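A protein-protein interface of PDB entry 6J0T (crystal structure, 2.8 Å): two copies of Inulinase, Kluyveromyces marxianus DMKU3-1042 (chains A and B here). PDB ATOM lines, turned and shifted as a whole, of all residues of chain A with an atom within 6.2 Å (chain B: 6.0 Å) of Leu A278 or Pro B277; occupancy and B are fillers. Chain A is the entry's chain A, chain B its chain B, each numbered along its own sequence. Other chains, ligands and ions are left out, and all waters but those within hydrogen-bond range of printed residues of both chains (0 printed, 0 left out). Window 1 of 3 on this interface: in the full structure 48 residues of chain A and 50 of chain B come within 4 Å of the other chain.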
ATOM      1  N   TRP A 232       0.910  17.748  31.912  1.00  0.00           N
ATOM      2  CA  TRP A 232       1.341  16.471  32.472  1.00  0.00           C
ATOM      3  C   TRP A 232       1.802  16.735  33.898  1.00  0.00           C
ATOM      4  O   TRP A 232       2.825  17.387  34.107  1.00  0.00           O
ATOM      5  CB  TRP A 232       2.462  15.859  31.630  1.00  0.00           C
ATOM      6  CG  TRP A 232       2.833  14.459  32.010  1.00  0.00           C
ATOM      7  CD1 TRP A 232       3.678  14.075  33.010  1.00  0.00           C
ATOM      8  CD2 TRP A 232       2.361  13.250  31.402  1.00  0.00           C
ATOM      9  NE1 TRP A 232       3.758  12.705  33.067  1.00  0.00           N
ATOM     10  CE2 TRP A 232       2.960  12.173  32.091  1.00  0.00           C
ATOM     11  CE3 TRP A 232       1.491  12.973  30.340  1.00  0.00           C
ATOM     12  CZ2 TRP A 232       2.727  10.834  31.747  1.00  0.00           C
ATOM     13  CZ3 TRP A 232       1.250  11.629  30.002  1.00  0.00           C
ATOM     14  CH2 TRP A 232       1.868  10.584  30.709  1.00  0.00           C
ATOM     15  N   GLY A 275       7.381  10.808  37.631  1.00  0.00           N
ATOM     16  CA  GLY A 275       6.132  10.649  36.909  1.00  0.00           C
ATOM     17  C   GLY A 275       6.139  10.976  35.425  1.00  0.00           C
ATOM     18  O   GLY A 275       5.077  10.908  34.801  1.00  0.00           O
ATOM     19  N   GLY A 276       7.282  11.331  34.838  1.00  0.00           N
ATOM     20  CA  GLY A 276       7.349  11.634  33.423  1.00  0.00           C
ATOM     21  C   GLY A 276       7.035  10.414  32.584  1.00  0.00           C
ATOM     22  O   GLY A 276       7.225   9.275  33.026  1.00  0.00           O
ATOM     23  N   PRO A 277       6.565  10.624  31.351  1.00  0.00           N
ATOM     24  CA  PRO A 277       6.025   9.494  30.568  1.00  0.00           C
ATOM     25  C   PRO A 277       7.062   8.468  30.150  1.00  0.00           C
ATOM     26  O   PRO A 277       6.692   7.322  29.886  1.00  0.00           O
ATOM     27  CB  PRO A 277       5.407  10.174  29.347  1.00  0.00           C
ATOM     28  CG  PRO A 277       6.253  11.388  29.174  1.00  0.00           C
ATOM     29  CD  PRO A 277       6.613  11.864  30.564  1.00  0.00           C
ATOM     30  N   LEU A 278       8.336   8.818  30.065  1.00  0.00           N
ATOM     31  CA  LEU A 278       9.325   7.771  29.854  1.00  0.00           C
ATOM     32  C   LEU A 278       9.809   7.179  31.165  1.00  0.00           C
ATOM     33  O   LEU A 278      10.431   6.106  31.156  1.00  0.00           O
ATOM     34  CB  LEU A 278      10.533   8.290  29.057  1.00  0.00           C
ATOM     35  CG  LEU A 278      10.206   8.812  27.645  1.00  0.00           C
ATOM     36  CD1 LEU A 278      11.437   9.392  26.982  1.00  0.00           C
ATOM     37  CD2 LEU A 278       9.599   7.746  26.769  1.00  0.00           C
ATOM     38  N   GLY A 279       9.497   7.824  32.281  1.00  0.00           N
ATOM     39  CA  GLY A 279      10.016   7.447  33.581  1.00  0.00           C
ATOM     40  C   GLY A 279      10.705   8.668  34.158  1.00  0.00           C
ATOM     41  O   GLY A 279      11.440   9.383  33.468  1.00  0.00           O
ATOM     42  N   GLY A 280      10.463   8.927  35.416  1.00  0.00           N
ATOM     43  CA  GLY A 280      11.264   9.950  36.059  1.00  0.00           C
ATOM     44  C   GLY A 280      10.992  11.327  35.477  1.00  0.00           C
ATOM     45  O   GLY A 280       9.839  11.710  35.212  1.00  0.00           O
ATOM     46  N   SER A 281      12.062  12.083  35.261  1.00  0.00           N
ATOM     47  CA  SER A 281      11.917  13.508  35.020  1.00  0.00           C
ATOM     48  C   SER A 281      11.682  13.822  33.545  1.00  0.00           C
ATOM     49  O   SER A 281      11.997  13.031  32.649  1.00  0.00           O
ATOM     50  CB  SER A 281      13.138  14.246  35.538  1.00  0.00           C
ATOM     51  OG  SER A 281      14.296  13.490  35.261  1.00  0.00           O
ATOM     52  N   PHE A 304       6.124  18.887  25.424  1.00  0.00           N
ATOM     53  CA  PHE A 304       7.412  18.599  26.024  1.00  0.00           C
ATOM     54  C   PHE A 304       8.496  19.399  25.309  1.00  0.00           C
ATOM     55  O   PHE A 304       8.415  19.630  24.098  1.00  0.00           O
ATOM     56  CB  PHE A 304       7.697  17.101  25.966  1.00  0.00           C
ATOM     57  CG  PHE A 304       6.873  16.321  26.917  1.00  0.00           C
ATOM     58  CD1 PHE A 304       6.136  16.964  27.881  1.00  0.00           C
ATOM     59  CD2 PHE A 304       6.813  14.956  26.849  1.00  0.00           C
ATOM     60  CE1 PHE A 304       5.347  16.251  28.773  1.00  0.00           C
ATOM     61  CE2 PHE A 304       6.031  14.251  27.739  1.00  0.00           C
ATOM     62  CZ  PHE A 304       5.302  14.908  28.707  1.00  0.00           C
ATOM     63  N   MET A 307      12.243  15.349  23.779  1.00  0.00           N
ATOM     64  CA  MET A 307      11.638  14.044  23.632  1.00  0.00           C
ATOM     65  C   MET A 307      12.579  12.945  24.060  1.00  0.00           C
ATOM     66  O   MET A 307      12.329  11.773  23.769  1.00  0.00           O
ATOM     67  CB  MET A 307      11.203  13.830  22.181  1.00  0.00           C
ATOM     68  CG  MET A 307      10.329  14.956  21.659  1.00  0.00           C
ATOM     69  SD  MET A 307       8.964  15.241  22.788  1.00  0.00           S
ATOM     70  CE  MET A 307       7.960  13.787  22.398  1.00  0.00           C
ATOM     71  N   GLY A 308      13.680  13.294  24.704  1.00  0.00           N
ATOM     72  CA  GLY A 308      14.612  12.309  25.200  1.00  0.00           C
ATOM     73  C   GLY A 308      14.449  12.115  26.693  1.00  0.00           C
ATOM     74  O   GLY A 308      13.762  12.866  27.379  1.00  0.00           O
ATOM     75  N   LYS A 309      15.103  11.084  27.199  1.00  0.00           N
ATOM     76  CA  LYS A 309      14.988  10.805  28.621  1.00  0.00           C
ATOM     77  C   LYS A 309      15.864  11.683  29.503  1.00  0.00           C
ATOM     78  O   LYS A 309      15.617  11.729  30.711  1.00  0.00           O
ATOM     79  CB  LYS A 309      15.332   9.353  28.899  1.00  0.00           C
ATOM     80  CG  LYS A 309      14.150   8.537  29.236  1.00  0.00           C
ATOM     81  CD  LYS A 309      14.470   7.512  30.288  1.00  0.00           C
ATOM     82  CE  LYS A 309      13.255   7.110  31.066  1.00  0.00           C
ATOM     83  NZ  LYS A 309      13.603   6.015  32.021  1.00  0.00           N
ATOM     84  N   ASN A 334      18.538  12.012  34.126  1.00  0.00           N
ATOM     85  CA  ASN A 334      17.176  11.725  34.593  1.00  0.00           C
ATOM     86  C   ASN A 334      17.285  11.255  36.023  1.00  0.00           C
ATOM     87  O   ASN A 334      18.099  10.447  36.238  1.00  0.00           O
ATOM     88  CB  ASN A 334      16.582  10.624  33.741  1.00  0.00           C
ATOM     89  CG  ASN A 334      15.171  10.314  34.135  1.00  0.00           C
ATOM     90  OD1 ASN A 334      14.939   9.886  35.236  1.00  0.00           O
ATOM     91  ND2 ASN A 334      14.245  10.522  33.241  1.00  0.00           N
ATOM     92  N   GLN A 336      15.775   8.985  37.731  1.00  0.00           N
ATOM     93  CA  GLN A 336      15.692   7.527  37.908  1.00  0.00           C
ATOM     94  C   GLN A 336      17.082   6.909  37.945  1.00  0.00           C
ATOM     95  O   GLN A 336      17.252   5.949  38.645  1.00  0.00           O
ATOM     96  CB  GLN A 336      14.924   6.931  36.742  1.00  0.00           C
ATOM     97  CG  GLN A 336      13.440   7.187  36.779  1.00  0.00           C
ATOM     98  CD  GLN A 336      12.719   6.266  35.846  1.00  0.00           C
ATOM     99  OE1 GLN A 336      13.039   6.165  34.686  1.00  0.00           O
ATOM    100  NE2 GLN A 336      11.727   5.584  36.353  1.00  0.00           N
ATOM    101  N   PHE A 478      16.111   1.296  33.952  1.00  0.00           N
ATOM    102  CA  PHE A 478      15.434   2.520  33.531  1.00  0.00           C
ATOM    103  C   PHE A 478      16.229   3.305  32.493  1.00  0.00           C
ATOM    104  O   PHE A 478      15.686   4.229  31.887  1.00  0.00           O
ATOM    105  CB  PHE A 478      15.130   3.426  34.734  1.00  0.00           C
ATOM    106  CG  PHE A 478      14.310   2.763  35.830  1.00  0.00           C
ATOM    107  CD1 PHE A 478      13.053   2.239  35.565  1.00  0.00           C
ATOM    108  CD2 PHE A 478      14.795   2.690  37.140  1.00  0.00           C
ATOM    109  CE1 PHE A 478      12.288   1.645  36.583  1.00  0.00           C
ATOM    110  CE2 PHE A 478      14.044   2.099  38.152  1.00  0.00           C
ATOM    111  CZ  PHE A 478      12.788   1.575  37.870  1.00  0.00           C
ATOM    112  N   ASN A 480      16.817   3.219  29.225  1.00  0.00           N
ATOM    113  CA  ASN A 480      16.247   2.493  28.093  1.00  0.00           C
ATOM    114  C   ASN A 480      17.246   2.419  26.964  1.00  0.00           C
ATOM    115  O   ASN A 480      17.913   3.404  26.633  1.00  0.00           O
ATOM    116  CB  ASN A 480      14.987   3.145  27.542  1.00  0.00           C
ATOM    117  CG  ASN A 480      14.198   3.867  28.579  1.00  0.00           C
ATOM    118  OD1 ASN A 480      14.138   5.093  28.564  1.00  0.00           O
ATOM    119  ND2 ASN A 480      13.569   3.123  29.482  1.00  0.00           N
ATOM    120  N   LEU A 483      15.166   4.491  22.079  1.00  0.00           N
ATOM    121  CA  LEU A 483      14.423   5.739  22.152  1.00  0.00           C
ATOM    122  C   LEU A 483      13.948   6.117  20.761  1.00  0.00           C
ATOM    123  O   LEU A 483      14.575   5.782  19.755  1.00  0.00           O
ATOM    124  CB  LEU A 483      15.258   6.885  22.730  1.00  0.00           C
ATOM    125  CG  LEU A 483      15.792   6.622  24.140  1.00  0.00           C
ATOM    126  CD1 LEU A 483      17.207   7.138  24.278  1.00  0.00           C
ATOM    127  CD2 LEU A 483      14.874   7.233  25.219  1.00  0.00           C
ATOM    128  N   ALA A 484      12.830   6.809  20.704  1.00  0.00           N
ATOM    129  CA  ALA A 484      12.245   7.125  19.419  1.00  0.00           C
ATOM    130  C   ALA A 484      11.819   8.580  19.401  1.00  0.00           C
ATOM    131  O   ALA A 484      11.546   9.185  20.441  1.00  0.00           O
ATOM    132  CB  ALA A 484      11.052   6.220  19.098  1.00  0.00           C
ATOM    133  N   ASN A 521      19.925  12.565  25.000  1.00  0.00           N
ATOM    134  CA  ASN A 521      20.129  11.348  25.771  1.00  0.00           C
ATOM    135  C   ASN A 521      21.614  11.165  26.042  1.00  0.00           C
ATOM    136  O   ASN A 521      22.456  11.753  25.366  1.00  0.00           O
ATOM    137  CB  ASN A 521      19.544  10.129  25.061  1.00  0.00           C
ATOM    138  CG  ASN A 521      18.100  10.337  24.671  1.00  0.00           C
ATOM    139  OD1 ASN A 521      17.199  10.147  25.478  1.00  0.00           O
ATOM    140  ND2 ASN A 521      17.872  10.738  23.421  1.00  0.00           N
ATOM    141  N   TRP B 232      -2.686  15.510  24.436  1.00  0.00           N
ATOM    142  CA  TRP B 232      -1.512  15.080  23.686  1.00  0.00           C
ATOM    143  C   TRP B 232      -1.924  14.941  22.230  1.00  0.00           C
ATOM    144  O   TRP B 232      -2.464  13.913  21.820  1.00  0.00           O
ATOM    145  CB  TRP B 232      -0.972  13.765  24.233  1.00  0.00           C
ATOM    146  CG  TRP B 232       0.334  13.360  23.633  1.00  0.00           C
ATOM    147  CD1 TRP B 232       0.534  12.606  22.508  1.00  0.00           C
ATOM    148  CD2 TRP B 232       1.631  13.701  24.124  1.00  0.00           C
ATOM    149  NE1 TRP B 232       1.883  12.451  22.273  1.00  0.00           N
ATOM    150  CE2 TRP B 232       2.577  13.118  23.248  1.00  0.00           C
ATOM    151  CE3 TRP B 232       2.088  14.437  25.227  1.00  0.00           C
ATOM    152  CZ2 TRP B 232       3.954  13.252  23.441  1.00  0.00           C
ATOM    153  CZ3 TRP B 232       3.463  14.573  25.419  1.00  0.00           C
ATOM    154  CH2 TRP B 232       4.378  13.987  24.523  1.00  0.00           C
ATOM    155  N   GLY B 275       2.798   9.508  17.077  1.00  0.00           N
ATOM    156  CA  GLY B 275       3.188  10.571  17.965  1.00  0.00           C
ATOM    157  C   GLY B 275       2.997  10.305  19.435  1.00  0.00           C
ATOM    158  O   GLY B 275       2.997  11.265  20.218  1.00  0.00           O
ATOM    159  N   GLY B 276       2.834   9.053  19.844  1.00  0.00           N
ATOM    160  CA  GLY B 276       2.829   8.742  21.251  1.00  0.00           C
ATOM    161  C   GLY B 276       4.190   9.026  21.856  1.00  0.00           C
ATOM    162  O   GLY B 276       5.219   9.006  21.165  1.00  0.00           O
ATOM    163  N   PRO B 277       4.224   9.294  23.165  1.00  0.00           N
ATOM    164  CA  PRO B 277       5.510   9.626  23.806  1.00  0.00           C
ATOM    165  C   PRO B 277       6.501   8.479  23.791  1.00  0.00           C
ATOM    166  O   PRO B 277       7.700   8.700  23.561  1.00  0.00           O
ATOM    167  CB  PRO B 277       5.103  10.027  25.232  1.00  0.00           C
ATOM    168  CG  PRO B 277       3.799   9.341  25.452  1.00  0.00           C
ATOM    169  CD  PRO B 277       3.104   9.303  24.118  1.00  0.00           C
ATOM    170  N   LEU B 278       6.034   7.252  24.017  1.00  0.00           N
ATOM    171  CA  LEU B 278       6.874   6.075  23.799  1.00  0.00           C
ATOM    172  C   LEU B 278       7.121   5.807  22.317  1.00  0.00           C
ATOM    173  O   LEU B 278       7.985   4.983  21.985  1.00  0.00           O
ATOM    174  CB  LEU B 278       6.235   4.850  24.456  1.00  0.00           C
ATOM    175  CG  LEU B 278       6.119   4.875  25.985  1.00  0.00           C
ATOM    176  CD1 LEU B 278       5.534   3.581  26.512  1.00  0.00           C
ATOM    177  CD2 LEU B 278       7.471   5.120  26.598  1.00  0.00           C
ATOM    178  N   GLY B 279       6.423   6.519  21.429  1.00  0.00           N
ATOM    179  CA  GLY B 279       6.532   6.319  20.002  1.00  0.00           C
ATOM    180  C   GLY B 279       5.376   5.501  19.529  1.00  0.00           C
ATOM    181  O   GLY B 279       5.019   4.517  20.174  1.00  0.00           O
ATOM    182  N   GLY B 280       4.744   5.899  18.436  1.00  0.00           N
ATOM    183  CA  GLY B 280       3.654   5.109  17.881  1.00  0.00           C
ATOM    184  C   GLY B 280       2.334   5.529  18.479  1.00  0.00           C
ATOM    185  O   GLY B 280       2.045   6.714  18.566  1.00  0.00           O
ATOM    186  N   SER B 281       1.546   4.557  18.912  1.00  0.00           N
ATOM    187  CA  SER B 281       0.166   4.801  19.296  1.00  0.00           C
ATOM    188  C   SER B 281       0.006   4.907  20.808  1.00  0.00           C
ATOM    189  O   SER B 281       0.827   4.407  21.575  1.00  0.00           O
ATOM    190  CB  SER B 281      -0.716   3.697  18.732  1.00  0.00           C
ATOM    191  OG  SER B 281      -0.040   2.454  18.725  1.00  0.00           O
ATOM    192  N   VAL B 282      -1.065   5.582  21.231  1.00  0.00           N
ATOM    193  CA  VAL B 282      -1.364   5.752  22.652  1.00  0.00           C
ATOM    194  C   VAL B 282      -2.822   6.184  22.788  1.00  0.00           C
ATOM    195  O   VAL B 282      -3.437   6.653  21.828  1.00  0.00           O
ATOM    196  CB  VAL B 282      -0.403   6.782  23.298  1.00  0.00           C
ATOM    197  CG1 VAL B 282      -0.568   8.122  22.607  1.00  0.00           C
ATOM    198  CG2 VAL B 282      -0.600   6.902  24.838  1.00  0.00           C
ATOM    199  N   PHE B 304      -3.236   9.535  30.457  1.00  0.00           N
ATOM    200  CA  PHE B 304      -3.136   8.370  29.593  1.00  0.00           C
ATOM    201  C   PHE B 304      -3.916   7.225  30.218  1.00  0.00           C
ATOM    202  O   PHE B 304      -3.825   6.978  31.424  1.00  0.00           O
ATOM    203  CB  PHE B 304      -1.679   7.941  29.377  1.00  0.00           C
ATOM    204  CG  PHE B 304      -0.924   8.770  28.360  1.00  0.00           C
ATOM    205  CD1 PHE B 304      -1.592   9.540  27.410  1.00  0.00           C
ATOM    206  CD2 PHE B 304       0.453   8.780  28.358  1.00  0.00           C
ATOM    207  CE1 PHE B 304      -0.893  10.313  26.481  1.00  0.00           C
ATOM    208  CE2 PHE B 304       1.152   9.529  27.437  1.00  0.00           C
ATOM    209  CZ  PHE B 304       0.477  10.301  26.493  1.00  0.00           C
ATOM    210  N   ALA B 484       8.492   1.188  31.932  1.00  0.00           N
ATOM    211  CA  ALA B 484       8.465   1.666  33.302  1.00  0.00           C
ATOM    212  C   ALA B 484       7.093   2.243  33.608  1.00  0.00           C
ATOM    213  O   ALA B 484       6.337   2.636  32.714  1.00  0.00           O
ATOM    214  CB  ALA B 484       9.552   2.719  33.556  1.00  0.00           C
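O of Gly B275 is in hydrogen-bond range of NE1 of Trp B232 (2.6 Å).
NE1 of Trp A232 lies within hydrogen-bond range of O of Gly A275 (2.8 Å).
NZ of Lys A309 sits close to O of Leu A278 (3.3 Å).
Among the printed residues, pairs that only touch across the chains: Trp A232 with Phe B304 (3.3 Å), Leu A278 with Leu B278 (3.4 Å), Phe A304 with Trp B232 (3.5 Å) and Leu A278 with Pro B277 (3.8 Å).
Of the printed residues of chain B, Trp A232 touches Phe B304.
Of chain B, only Pro B277 and Leu B278 come within 4 Å of Leu A278.
Printed residues of chain B within 4 Å of Phe A304: Trp B232.
Of the printed residues of chain A, Trp B232 touches Phe A304 (3.5 Å).
Pro B277 touches one residue of chain A.
Of the printed residues of chain A, Phe B304 touches Trp A232 (3.3 Å).
The nearest residue of chain B that does not touch Leu A278 is Ala B484 (4.2 Å).
Of the 11 printed residues of chain B, 4 touch a printed residue of chain A.
Among the printed residues, 4 pairs touch across the chains.
Among the printed residues, no Asp or Glu carboxylate lies within 4 Å of a Lys or Arg side-chain nitrogen of the other chain.
Trp A232 touches Phe B304, and with the chains exchanged Phe A304 touches Trp B232.
Leu A278 touches Pro B277, but with the chains exchanged Pro A277 does not touch Leu B278 (4.03 Å).
Leu A278 touches its own counterpart, Leu B278.
Of the 4 pairs that touch across the chains among the printed residues, 3 have their exchanged pair printed and touching as well.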
